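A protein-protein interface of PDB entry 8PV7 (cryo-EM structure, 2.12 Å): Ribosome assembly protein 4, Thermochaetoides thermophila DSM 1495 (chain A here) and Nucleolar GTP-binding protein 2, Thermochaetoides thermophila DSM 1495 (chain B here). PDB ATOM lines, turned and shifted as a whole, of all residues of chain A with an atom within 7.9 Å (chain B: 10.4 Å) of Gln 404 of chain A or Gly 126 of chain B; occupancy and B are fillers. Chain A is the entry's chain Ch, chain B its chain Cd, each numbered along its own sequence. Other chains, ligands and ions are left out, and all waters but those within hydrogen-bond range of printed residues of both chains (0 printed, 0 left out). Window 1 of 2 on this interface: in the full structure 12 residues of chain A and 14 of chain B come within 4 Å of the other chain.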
ATOM      1  N   ASP A 381     -30.780   0.909 -29.278  1.00  0.00           N
ATOM      2  CA  ASP A 381     -30.733  -0.535 -29.434  1.00  0.00           C
ATOM      3  C   ASP A 381     -29.721  -1.189 -28.504  1.00  0.00           C
ATOM      4  O   ASP A 381     -29.325  -2.329 -28.756  1.00  0.00           O
ATOM      5  CB  ASP A 381     -30.459  -0.917 -30.899  1.00  0.00           C
ATOM      6  CG  ASP A 381     -29.119  -0.412 -31.432  1.00  0.00           C
ATOM      7  OD1 ASP A 381     -28.285   0.131 -30.689  1.00  0.00           O
ATOM      8  OD2 ASP A 381     -28.886  -0.576 -32.642  1.00  0.00           O
ATOM      9  N   PHE A 382     -29.280  -0.458 -27.473  1.00  0.00           N
ATOM     10  CA  PHE A 382     -28.391  -0.864 -26.378  1.00  0.00           C
ATOM     11  C   PHE A 382     -26.937  -0.886 -26.818  1.00  0.00           C
ATOM     12  O   PHE A 382     -26.072  -1.319 -26.056  1.00  0.00           O
ATOM     13  CB  PHE A 382     -28.700  -2.237 -25.744  1.00  0.00           C
ATOM     14  CG  PHE A 382     -30.100  -2.412 -25.184  1.00  0.00           C
ATOM     15  CD1 PHE A 382     -31.081  -1.431 -25.266  1.00  0.00           C
ATOM     16  CD2 PHE A 382     -30.422  -3.599 -24.557  1.00  0.00           C
ATOM     17  CE1 PHE A 382     -32.331  -1.640 -24.750  1.00  0.00           C
ATOM     18  CE2 PHE A 382     -31.671  -3.810 -24.039  1.00  0.00           C
ATOM     19  CZ  PHE A 382     -32.625  -2.831 -24.131  1.00  0.00           C
ATOM     20  N   THR A 383     -26.634  -0.443 -28.033  1.00  0.00           N
ATOM     21  CA  THR A 383     -25.312  -0.652 -28.597  1.00  0.00           C
ATOM     22  C   THR A 383     -24.681   0.663 -29.016  1.00  0.00           C
ATOM     23  O   THR A 383     -25.279   1.749 -28.939  1.00  0.00           O
ATOM     24  CB  THR A 383     -25.321  -1.583 -29.821  1.00  0.00           C
ATOM     25  OG1 THR A 383     -25.720  -0.842 -30.978  1.00  0.00           O
ATOM     26  CG2 THR A 383     -26.245  -2.762 -29.630  1.00  0.00           C
ATOM     27  N   LEU A 401     -20.748  -3.580 -27.454  1.00  0.00           N
ATOM     28  CA  LEU A 401     -21.835  -4.369 -26.899  1.00  0.00           C
ATOM     29  C   LEU A 401     -21.587  -4.585 -25.416  1.00  0.00           C
ATOM     30  O   LEU A 401     -20.452  -4.767 -24.977  1.00  0.00           O
ATOM     31  CB  LEU A 401     -21.942  -5.743 -27.574  1.00  0.00           C
ATOM     32  CG  LEU A 401     -22.393  -5.878 -29.022  1.00  0.00           C
ATOM     33  CD1 LEU A 401     -22.245  -7.320 -29.458  1.00  0.00           C
ATOM     34  CD2 LEU A 401     -23.820  -5.443 -29.159  1.00  0.00           C
ATOM     35  N   GLY A 402     -22.668  -4.606 -24.650  1.00  0.00           N
ATOM     36  CA  GLY A 402     -22.591  -4.869 -23.234  1.00  0.00           C
ATOM     37  C   GLY A 402     -23.566  -4.094 -22.383  1.00  0.00           C
ATOM     38  O   GLY A 402     -23.894  -4.550 -21.284  1.00  0.00           O
ATOM     39  N   HIS A 403     -24.043  -2.949 -22.856  1.00  0.00           N
ATOM     40  CA  HIS A 403     -25.060  -2.211 -22.127  1.00  0.00           C
ATOM     41  C   HIS A 403     -26.377  -2.975 -22.174  1.00  0.00           C
ATOM     42  O   HIS A 403     -26.754  -3.531 -23.207  1.00  0.00           O
ATOM     43  CB  HIS A 403     -25.236  -0.823 -22.736  1.00  0.00           C
ATOM     44  CG  HIS A 403     -24.390   0.231 -22.097  1.00  0.00           C
ATOM     45  ND1 HIS A 403     -24.591   0.679 -20.811  1.00  0.00           N
ATOM     46  CD2 HIS A 403     -23.341   0.935 -22.580  1.00  0.00           C
ATOM     47  CE1 HIS A 403     -23.696   1.607 -20.526  1.00  0.00           C
ATOM     48  NE2 HIS A 403     -22.930   1.785 -21.586  1.00  0.00           N
ATOM     49  N   GLN A 404     -27.076  -3.005 -21.047  1.00  0.00           N
ATOM     50  CA  GLN A 404     -28.341  -3.717 -20.935  1.00  0.00           C
ATOM     51  C   GLN A 404     -29.551  -2.826 -21.176  1.00  0.00           C
ATOM     52  O   GLN A 404     -30.683  -3.289 -21.018  1.00  0.00           O
ATOM     53  CB  GLN A 404     -28.458  -4.367 -19.556  1.00  0.00           C
ATOM     54  CG  GLN A 404     -27.267  -5.205 -19.141  1.00  0.00           C
ATOM     55  CD  GLN A 404     -27.112  -6.454 -19.971  1.00  0.00           C
ATOM     56  OE1 GLN A 404     -26.476  -6.441 -21.018  1.00  0.00           O
ATOM     57  NE2 GLN A 404     -27.708  -7.542 -19.511  1.00  0.00           N
ATOM     58  N   ASN A 405     -29.344  -1.566 -21.532  1.00  0.00           N
ATOM     59  CA  ASN A 405     -30.440  -0.657 -21.819  1.00  0.00           C
ATOM     60  C   ASN A 405     -29.918   0.395 -22.787  1.00  0.00           C
ATOM     61  O   ASN A 405     -28.795   0.296 -23.283  1.00  0.00           O
ATOM     62  CB  ASN A 405     -31.000  -0.055 -20.525  1.00  0.00           C
ATOM     63  CG  ASN A 405     -32.467   0.298 -20.634  1.00  0.00           C
ATOM     64  OD1 ASN A 405     -33.016   0.395 -21.727  1.00  0.00           O
ATOM     65  ND2 ASN A 405     -33.119   0.456 -19.496  1.00  0.00           N
ATOM     66  N   LYS A 406     -30.749   1.398 -23.061  1.00  0.00           N
ATOM     67  CA  LYS A 406     -30.429   2.419 -24.050  1.00  0.00           C
ATOM     68  C   LYS A 406     -29.194   3.218 -23.652  1.00  0.00           C
ATOM     69  O   LYS A 406     -28.977   3.506 -22.474  1.00  0.00           O
ATOM     70  CB  LYS A 406     -31.626   3.357 -24.219  1.00  0.00           C
ATOM     71  CG  LYS A 406     -32.926   2.630 -24.462  1.00  0.00           C
ATOM     72  CD  LYS A 406     -34.111   3.572 -24.549  1.00  0.00           C
ATOM     73  CE  LYS A 406     -34.406   4.229 -23.227  1.00  0.00           C
ATOM     74  NZ  LYS A 406     -34.850   3.221 -22.228  1.00  0.00           N
ATOM     75  N   VAL A 407     -28.372   3.559 -24.640  1.00  0.00           N
ATOM     76  CA  VAL A 407     -27.172   4.359 -24.419  1.00  0.00           C
ATOM     77  C   VAL A 407     -27.506   5.807 -24.732  1.00  0.00           C
ATOM     78  O   VAL A 407     -27.815   6.146 -25.879  1.00  0.00           O
ATOM     79  CB  VAL A 407     -25.991   3.872 -25.271  1.00  0.00           C
ATOM     80  CG1 VAL A 407     -24.688   4.433 -24.719  1.00  0.00           C
ATOM     81  CG2 VAL A 407     -25.945   2.361 -25.313  1.00  0.00           C
ATOM     82  N   GLY A 423     -25.450   4.792 -19.707  1.00  0.00           N
ATOM     83  CA  GLY A 423     -26.599   4.018 -20.114  1.00  0.00           C
ATOM     84  C   GLY A 423     -27.786   4.208 -19.186  1.00  0.00           C
ATOM     85  O   GLY A 423     -27.672   4.750 -18.088  1.00  0.00           O
ATOM     86  N   TRP A 424     -28.927   3.719 -19.654  1.00  0.00           N
ATOM     87  CA  TRP A 424     -30.159   3.682 -18.885  1.00  0.00           C
ATOM     88  C   TRP A 424     -30.246   2.460 -17.987  1.00  0.00           C
ATOM     89  O   TRP A 424     -31.269   2.265 -17.328  1.00  0.00           O
ATOM     90  CB  TRP A 424     -31.368   3.716 -19.818  1.00  0.00           C
ATOM     91  CG  TRP A 424     -31.630   5.039 -20.449  1.00  0.00           C
ATOM     92  CD1 TRP A 424     -30.775   5.761 -21.222  1.00  0.00           C
ATOM     93  CD2 TRP A 424     -32.834   5.798 -20.368  1.00  0.00           C
ATOM     94  NE1 TRP A 424     -31.370   6.921 -21.629  1.00  0.00           N
ATOM     95  CE2 TRP A 424     -32.637   6.972 -21.115  1.00  0.00           C
ATOM     96  CE3 TRP A 424     -34.061   5.603 -19.730  1.00  0.00           C
ATOM     97  CZ2 TRP A 424     -33.620   7.943 -21.250  1.00  0.00           C
ATOM     98  CZ3 TRP A 424     -35.035   6.569 -19.864  1.00  0.00           C
ATOM     99  CH2 TRP A 424     -34.809   7.726 -20.619  1.00  0.00           C
ATOM    100  N   ASP A 425     -29.212   1.621 -17.983  1.00  0.00           N
ATOM    101  CA  ASP A 425     -29.094   0.499 -17.067  1.00  0.00           C
ATOM    102  C   ASP A 425     -28.282   0.862 -15.830  1.00  0.00           C
ATOM    103  O   ASP A 425     -27.653  -0.014 -15.228  1.00  0.00           O
ATOM    104  CB  ASP A 425     -28.474  -0.705 -17.780  1.00  0.00           C
ATOM    105  CG  ASP A 425     -27.160  -0.370 -18.461  1.00  0.00           C
ATOM    106  OD1 ASP A 425     -26.799   0.820 -18.535  1.00  0.00           O
ATOM    107  OD2 ASP A 425     -26.480  -1.299 -18.927  1.00  0.00           O
ATOM    108  N   ASN A 426     -28.282   2.144 -15.457  1.00  0.00           N
ATOM    109  CA  ASN A 426     -27.589   2.713 -14.303  1.00  0.00           C
ATOM    110  C   ASN A 426     -26.085   2.494 -14.338  1.00  0.00           C
ATOM    111  O   ASN A 426     -25.456   2.402 -13.287  1.00  0.00           O
ATOM    112  CB  ASN A 426     -28.139   2.174 -12.974  1.00  0.00           C
ATOM    113  CG  ASN A 426     -29.620   1.906 -13.016  1.00  0.00           C
ATOM    114  OD1 ASN A 426     -30.339   2.449 -13.847  1.00  0.00           O
ATOM    115  ND2 ASN A 426     -30.084   1.045 -12.126  1.00  0.00           N
ATOM    116  N   SER A 427     -25.473   2.409 -15.514  1.00  0.00           N
ATOM    117  CA  SER A 427     -24.057   2.091 -15.585  1.00  0.00           C
ATOM    118  C   SER A 427     -23.350   2.956 -16.617  1.00  0.00           C
ATOM    119  O   SER A 427     -23.925   3.382 -17.623  1.00  0.00           O
ATOM    120  CB  SER A 427     -23.828   0.607 -15.905  1.00  0.00           C
ATOM    121  OG  SER A 427     -24.060   0.333 -17.271  1.00  0.00           O
ATOM    122  N   LYS A 429     -19.843   2.692 -18.907  1.00  0.00           N
ATOM    123  CA  LYS A 429     -18.900   1.699 -19.393  1.00  0.00           C
ATOM    124  C   LYS A 429     -17.723   2.369 -20.083  1.00  0.00           C
ATOM    125  O   LYS A 429     -17.854   3.461 -20.647  1.00  0.00           O
ATOM    126  CB  LYS A 429     -19.574   0.710 -20.339  1.00  0.00           C
ATOM    127  CG  LYS A 429     -20.486  -0.264 -19.631  1.00  0.00           C
ATOM    128  CD  LYS A 429     -21.062  -1.283 -20.581  1.00  0.00           C
ATOM    129  CE  LYS A 429     -21.717  -2.412 -19.815  1.00  0.00           C
ATOM    130  NZ  LYS A 429     -22.833  -1.946 -18.969  1.00  0.00           N
ATOM    131  N   ASP B 119     -24.568  -9.865  -9.467  1.00  0.00           N
ATOM    132  CA  ASP B 119     -24.109  -9.574 -10.814  1.00  0.00           C
ATOM    133  C   ASP B 119     -25.285  -9.521 -11.783  1.00  0.00           C
ATOM    134  O   ASP B 119     -26.265 -10.258 -11.658  1.00  0.00           O
ATOM    135  CB  ASP B 119     -23.099 -10.624 -11.274  1.00  0.00           C
ATOM    136  CG  ASP B 119     -21.898 -10.712 -10.361  1.00  0.00           C
ATOM    137  OD1 ASP B 119     -21.732 -11.753  -9.691  1.00  0.00           O
ATOM    138  OD2 ASP B 119     -21.119  -9.738 -10.313  1.00  0.00           O
ATOM    139  N   GLY B 120     -25.171  -8.634 -12.759  1.00  0.00           N
ATOM    140  CA  GLY B 120     -26.222  -8.436 -13.726  1.00  0.00           C
ATOM    141  C   GLY B 120     -26.324  -9.591 -14.695  1.00  0.00           C
ATOM    142  O   GLY B 120     -25.470 -10.489 -14.750  1.00  0.00           O
ATOM    143  N   PRO B 121     -27.409  -9.599 -15.465  1.00  0.00           N
ATOM    144  CA  PRO B 121     -27.578 -10.636 -16.488  1.00  0.00           C
ATOM    145  C   PRO B 121     -26.533 -10.512 -17.585  1.00  0.00           C
ATOM    146  O   PRO B 121     -25.922  -9.462 -17.794  1.00  0.00           O
ATOM    147  CB  PRO B 121     -28.984 -10.389 -17.045  1.00  0.00           C
ATOM    148  CG  PRO B 121     -29.634  -9.413 -16.152  1.00  0.00           C
ATOM    149  CD  PRO B 121     -28.654  -8.868 -15.176  1.00  0.00           C
ATOM    150  N   LYS B 122     -26.326 -11.626 -18.283  1.00  0.00           N
ATOM    151  CA  LYS B 122     -25.416 -11.649 -19.419  1.00  0.00           C
ATOM    152  C   LYS B 122     -25.976 -10.801 -20.555  1.00  0.00           C
ATOM    153  O   LYS B 122     -27.193 -10.645 -20.704  1.00  0.00           O
ATOM    154  CB  LYS B 122     -25.160 -13.085 -19.911  1.00  0.00           C
ATOM    155  CG  LYS B 122     -24.421 -14.072 -18.968  1.00  0.00           C
ATOM    156  CD  LYS B 122     -25.187 -14.512 -17.722  1.00  0.00           C
ATOM    157  CE  LYS B 122     -26.456 -15.258 -18.102  1.00  0.00           C
ATOM    158  NZ  LYS B 122     -27.549 -15.071 -17.106  1.00  0.00           N
ATOM    159  N   LEU B 123     -25.068 -10.244 -21.360  1.00  0.00           N
ATOM    160  CA  LEU B 123     -25.469  -9.279 -22.379  1.00  0.00           C
ATOM    161  C   LEU B 123     -26.271  -9.938 -23.497  1.00  0.00           C
ATOM    162  O   LEU B 123     -27.152  -9.305 -24.092  1.00  0.00           O
ATOM    163  CB  LEU B 123     -24.235  -8.560 -22.929  1.00  0.00           C
ATOM    164  CG  LEU B 123     -23.160  -9.347 -23.679  1.00  0.00           C
ATOM    165  CD1 LEU B 123     -23.321  -9.196 -25.185  1.00  0.00           C
ATOM    166  CD2 LEU B 123     -21.774  -8.913 -23.229  1.00  0.00           C
ATOM    167  N   GLU B 124     -25.984 -11.207 -23.789  1.00  0.00           N
ATOM    168  CA  GLU B 124     -26.728 -11.925 -24.819  1.00  0.00           C
ATOM    169  C   GLU B 124     -28.194 -12.077 -24.431  1.00  0.00           C
ATOM    170  O   GLU B 124     -29.095 -11.790 -25.227  1.00  0.00           O
ATOM    171  CB  GLU B 124     -26.092 -13.296 -25.068  1.00  0.00           C
ATOM    172  CG  GLU B 124     -24.574 -13.286 -25.249  1.00  0.00           C
ATOM    173  CD  GLU B 124     -23.812 -13.403 -23.936  1.00  0.00           C
ATOM    174  OE1 GLU B 124     -24.263 -14.156 -23.047  1.00  0.00           O
ATOM    175  OE2 GLU B 124     -22.762 -12.743 -23.792  1.00  0.00           O
ATOM    176  N   ASP B 125     -28.447 -12.493 -23.187  1.00  0.00           N
ATOM    177  CA  ASP B 125     -29.818 -12.580 -22.699  1.00  0.00           C
ATOM    178  C   ASP B 125     -30.447 -11.200 -22.564  1.00  0.00           C
ATOM    179  O   ASP B 125     -31.648 -11.038 -22.799  1.00  0.00           O
ATOM    180  CB  ASP B 125     -29.857 -13.320 -21.364  1.00  0.00           C
ATOM    181  CG  ASP B 125     -29.113 -14.636 -21.409  1.00  0.00           C
ATOM    182  OD1 ASP B 125     -28.640 -15.015 -22.501  1.00  0.00           O
ATOM    183  OD2 ASP B 125     -28.999 -15.292 -20.353  1.00  0.00           O
ATOM    184  N   GLY B 126     -29.648 -10.190 -22.207  1.00  0.00           N
ATOM    185  CA  GLY B 126     -30.186  -8.844 -22.076  1.00  0.00           C
ATOM    186  C   GLY B 126     -30.657  -8.252 -23.393  1.00  0.00           C
ATOM    187  O   GLY B 126     -31.657  -7.534 -23.438  1.00  0.00           O
ATOM    188  N   LEU B 127     -29.932  -8.529 -24.478  1.00  0.00           N
ATOM    189  CA  LEU B 127     -30.356  -8.066 -25.798  1.00  0.00           C
ATOM    190  C   LEU B 127     -31.473  -8.937 -26.369  1.00  0.00           C
ATOM    191  O   LEU B 127     -32.393  -8.427 -27.030  1.00  0.00           O
ATOM    192  CB  LEU B 127     -29.156  -8.032 -26.741  1.00  0.00           C
ATOM    193  CG  LEU B 127     -28.557  -6.647 -26.992  1.00  0.00           C
ATOM    194  CD1 LEU B 127     -27.243  -6.762 -27.737  1.00  0.00           C
ATOM    195  CD2 LEU B 127     -29.529  -5.780 -27.767  1.00  0.00           C
ATOM    196  N   LYS B 128     -31.411 -10.248 -26.113  1.00  0.00           N
ATOM    197  CA  LYS B 128     -32.447 -11.162 -26.573  1.00  0.00           C
ATOM    198  C   LYS B 128     -33.785 -10.863 -25.910  1.00  0.00           C
ATOM    199  O   LYS B 128     -34.839 -10.989 -26.541  1.00  0.00           O
ATOM    200  CB  LYS B 128     -32.017 -12.602 -26.293  1.00  0.00           C
ATOM    201  CG  LYS B 128     -33.047 -13.655 -26.650  1.00  0.00           C
ATOM    202  CD  LYS B 128     -33.000 -14.820 -25.682  1.00  0.00           C
ATOM    203  CE  LYS B 128     -33.244 -16.134 -26.397  1.00  0.00           C
ATOM    204  NZ  LYS B 128     -32.074 -16.534 -27.222  1.00  0.00           N
ATOM    205  N   LYS B 129     -33.760 -10.434 -24.649  1.00  0.00           N
ATOM    206  CA  LYS B 129     -34.993 -10.212 -23.912  1.00  0.00           C
ATOM    207  C   LYS B 129     -35.712  -8.951 -24.378  1.00  0.00           C
ATOM    208  O   LYS B 129     -36.875  -8.747 -24.021  1.00  0.00           O
ATOM    209  CB  LYS B 129     -34.675 -10.152 -22.412  1.00  0.00           C
ATOM    210  CG  LYS B 129     -35.864 -10.350 -21.477  1.00  0.00           C
ATOM    211  CD  LYS B 129     -35.851  -9.386 -20.303  1.00  0.00           C
ATOM    212  CE  LYS B 129     -36.426  -8.032 -20.679  1.00  0.00           C
ATOM    213  NZ  LYS B 129     -37.657  -8.140 -21.509  1.00  0.00           N
ATOM    214  N   HIS B 130     -35.053  -8.107 -25.170  1.00  0.00           N
ATOM    215  CA  HIS B 130     -35.660  -6.889 -25.685  1.00  0.00           C
ATOM    216  C   HIS B 130     -35.756  -6.842 -27.202  1.00  0.00           C
ATOM    217  O   HIS B 130     -36.302  -5.867 -27.733  1.00  0.00           O
ATOM    218  CB  HIS B 130     -34.886  -5.659 -25.196  1.00  0.00           C
ATOM    219  CG  HIS B 130     -34.956  -5.449 -23.717  1.00  0.00           C
ATOM    220  ND1 HIS B 130     -35.971  -4.738 -23.117  1.00  0.00           N
ATOM    221  CD2 HIS B 130     -34.134  -5.848 -22.719  1.00  0.00           C
ATOM    222  CE1 HIS B 130     -35.773  -4.709 -21.813  1.00  0.00           C
ATOM    223  NE2 HIS B 130     -34.662  -5.372 -21.545  1.00  0.00           N
ATOM    224  N   GLN B 131     -35.226  -7.851 -27.905  1.00  0.00           N
ATOM    225  CA  GLN B 131     -35.237  -7.846 -29.368  1.00  0.00           C
ATOM    226  C   GLN B 131     -36.648  -7.786 -29.956  1.00  0.00           C
ATOM    227  O   GLN B 131     -36.873  -7.102 -30.959  1.00  0.00           O
ATOM    228  CB  GLN B 131     -34.498  -9.072 -29.891  1.00  0.00           C
ATOM    229  CG  GLN B 131     -33.596  -8.781 -31.064  1.00  0.00           C
ATOM    230  CD  GLN B 131     -32.659  -7.618 -30.808  1.00  0.00           C
ATOM    231  OE1 GLN B 131     -31.896  -7.619 -29.843  1.00  0.00           O
ATOM    232  NE2 GLN B 131     -32.719  -6.612 -31.671  1.00  0.00           N
ATOM    233  N   ALA B 132     -37.610  -8.485 -29.349  1.00  0.00           N
ATOM    234  CA  ALA B 132     -38.963  -8.525 -29.902  1.00  0.00           C
ATOM    235  C   ALA B 132     -39.649  -7.165 -29.809  1.00  0.00           C
ATOM    236  O   ALA B 132     -40.235  -6.677 -30.787  1.00  0.00           O
ATOM    237  CB  ALA B 132     -39.783  -9.595 -29.185  1.00  0.00           C
ATOM    238  N   LYS B 133     -39.584  -6.537 -28.636  1.00  0.00           N
ATOM    239  CA  LYS B 133     -40.172  -5.215 -28.456  1.00  0.00           C
ATOM    240  C   LYS B 133     -39.430  -4.174 -29.279  1.00  0.00           C
ATOM    241  O   LYS B 133     -40.040  -3.222 -29.772  1.00  0.00           O
ATOM    242  CB  LYS B 133     -40.220  -4.790 -26.974  1.00  0.00           C
ATOM    243  CG  LYS B 133     -40.989  -5.641 -25.893  1.00  0.00           C
ATOM    244  CD  LYS B 133     -40.818  -7.169 -25.807  1.00  0.00           C
ATOM    245  CE  LYS B 133     -39.365  -7.582 -25.645  1.00  0.00           C
ATOM    246  NZ  LYS B 133     -39.194  -9.057 -25.637  1.00  0.00           N
ATOM    247  N   MET B 134     -38.122  -4.364 -29.478  1.00  0.00           N
ATOM    248  CA  MET B 134     -37.372  -3.488 -30.368  1.00  0.00           C
ATOM    249  C   MET B 134     -37.869  -3.587 -31.806  1.00  0.00           C
ATOM    250  O   MET B 134     -38.041  -2.564 -32.476  1.00  0.00           O
ATOM    251  CB  MET B 134     -35.890  -3.834 -30.306  1.00  0.00           C
ATOM    252  CG  MET B 134     -34.961  -2.695 -30.617  1.00  0.00           C
ATOM    253  SD  MET B 134     -33.420  -2.881 -29.713  1.00  0.00           S
ATOM    254  CE  MET B 134     -33.996  -3.012 -28.021  1.00  0.00           C
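O of Pro 121 of chain B lies within hydrogen-bond range of NE2 of Gln 404 of chain A (3.1 Å).
The backbone carbonyl oxygen (O) of Lys 122 of chain B lies within hydrogen-bond range of the side-chain amide nitrogen (NE2) of Gln 404 of chain A.
NZ of Lys 122 of chain B is in salt-bridge range of OD2 of Asp 125 of chain B, at 3.6 Å.
O of Gly 402 of chain A lies close to OE1 of Gln 404 of chain A (3.2 Å).
The side-chain carboxylate (OD1) of Asp 381 of chain A is in hydrogen-bond range of the side-chain hydroxyl (OG1) of Thr 383 of chain A.
OE1 of Gln 131 of chain B lies close to O of Leu 127 of chain B (3.0 Å).
N of Gln 404 of chain A sits at hydrogen-bond distance from OD2 of Asp 425 of chain A, 2.8 Å away.
Leu 127 of chain B touches Asp 381 of chain A.
CA of Asp 381 of chain A touches SD of Met 134 of chain B (3.6 Å).
Phe 382 of chain A touches Gly 126 of chain B.
Phe 382 of chain A touches Leu 127 of chain B (CD2 to CD2, 3.98 Å).
CE2 of Phe 382 of chain A touches CD2 of His 130 of chain B (3.5 Å).
Met 134 of chain B touches Phe 382 of chain A (CE to CE1, 3.9 Å).
CD2 of Leu 401 of chain A touches CD1 of Leu 127 of chain B, at 3.9 Å.
OE1 of Gln 404 of chain A touches CA of Leu 123 of chain B, 3.3 Å away.
NE2 of Gln 404 of chain A touches CA of Gly 126 of chain B, at 3.8 Å.
Of the printed residues of chain B, Asp 381 of chain A touches Leu 127 (3.6 Å) and Met 134 (3.6 Å).
Of the printed residues of chain B, Phe 382 of chain A touches Gly 126, Leu 127, His 130 and Met 134.
Of the printed residues of chain B, Leu 401 of chain A touches Leu 127.
No residue of chain B comes within 4 Å of Gly 402 of chain A.
Gln 404 of chain A touches just these residues of chain B: Pro 121, Lys 122, Leu 123 and Gly 126.
Of the printed residues of chain A, Leu 127 of chain B touches Asp 381, Phe 382 and Leu 401.
Of the printed residues of chain A, His 130 of chain B touches Phe 382 (3.5 Å).
The nearest residue of chain B that does not touch Gln 404 of chain A is His 130 of chain B (4.5 Å).
The nearest residue of chain A that does not touch Gly 126 of chain B is His 403 of chain A (6.1 Å).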
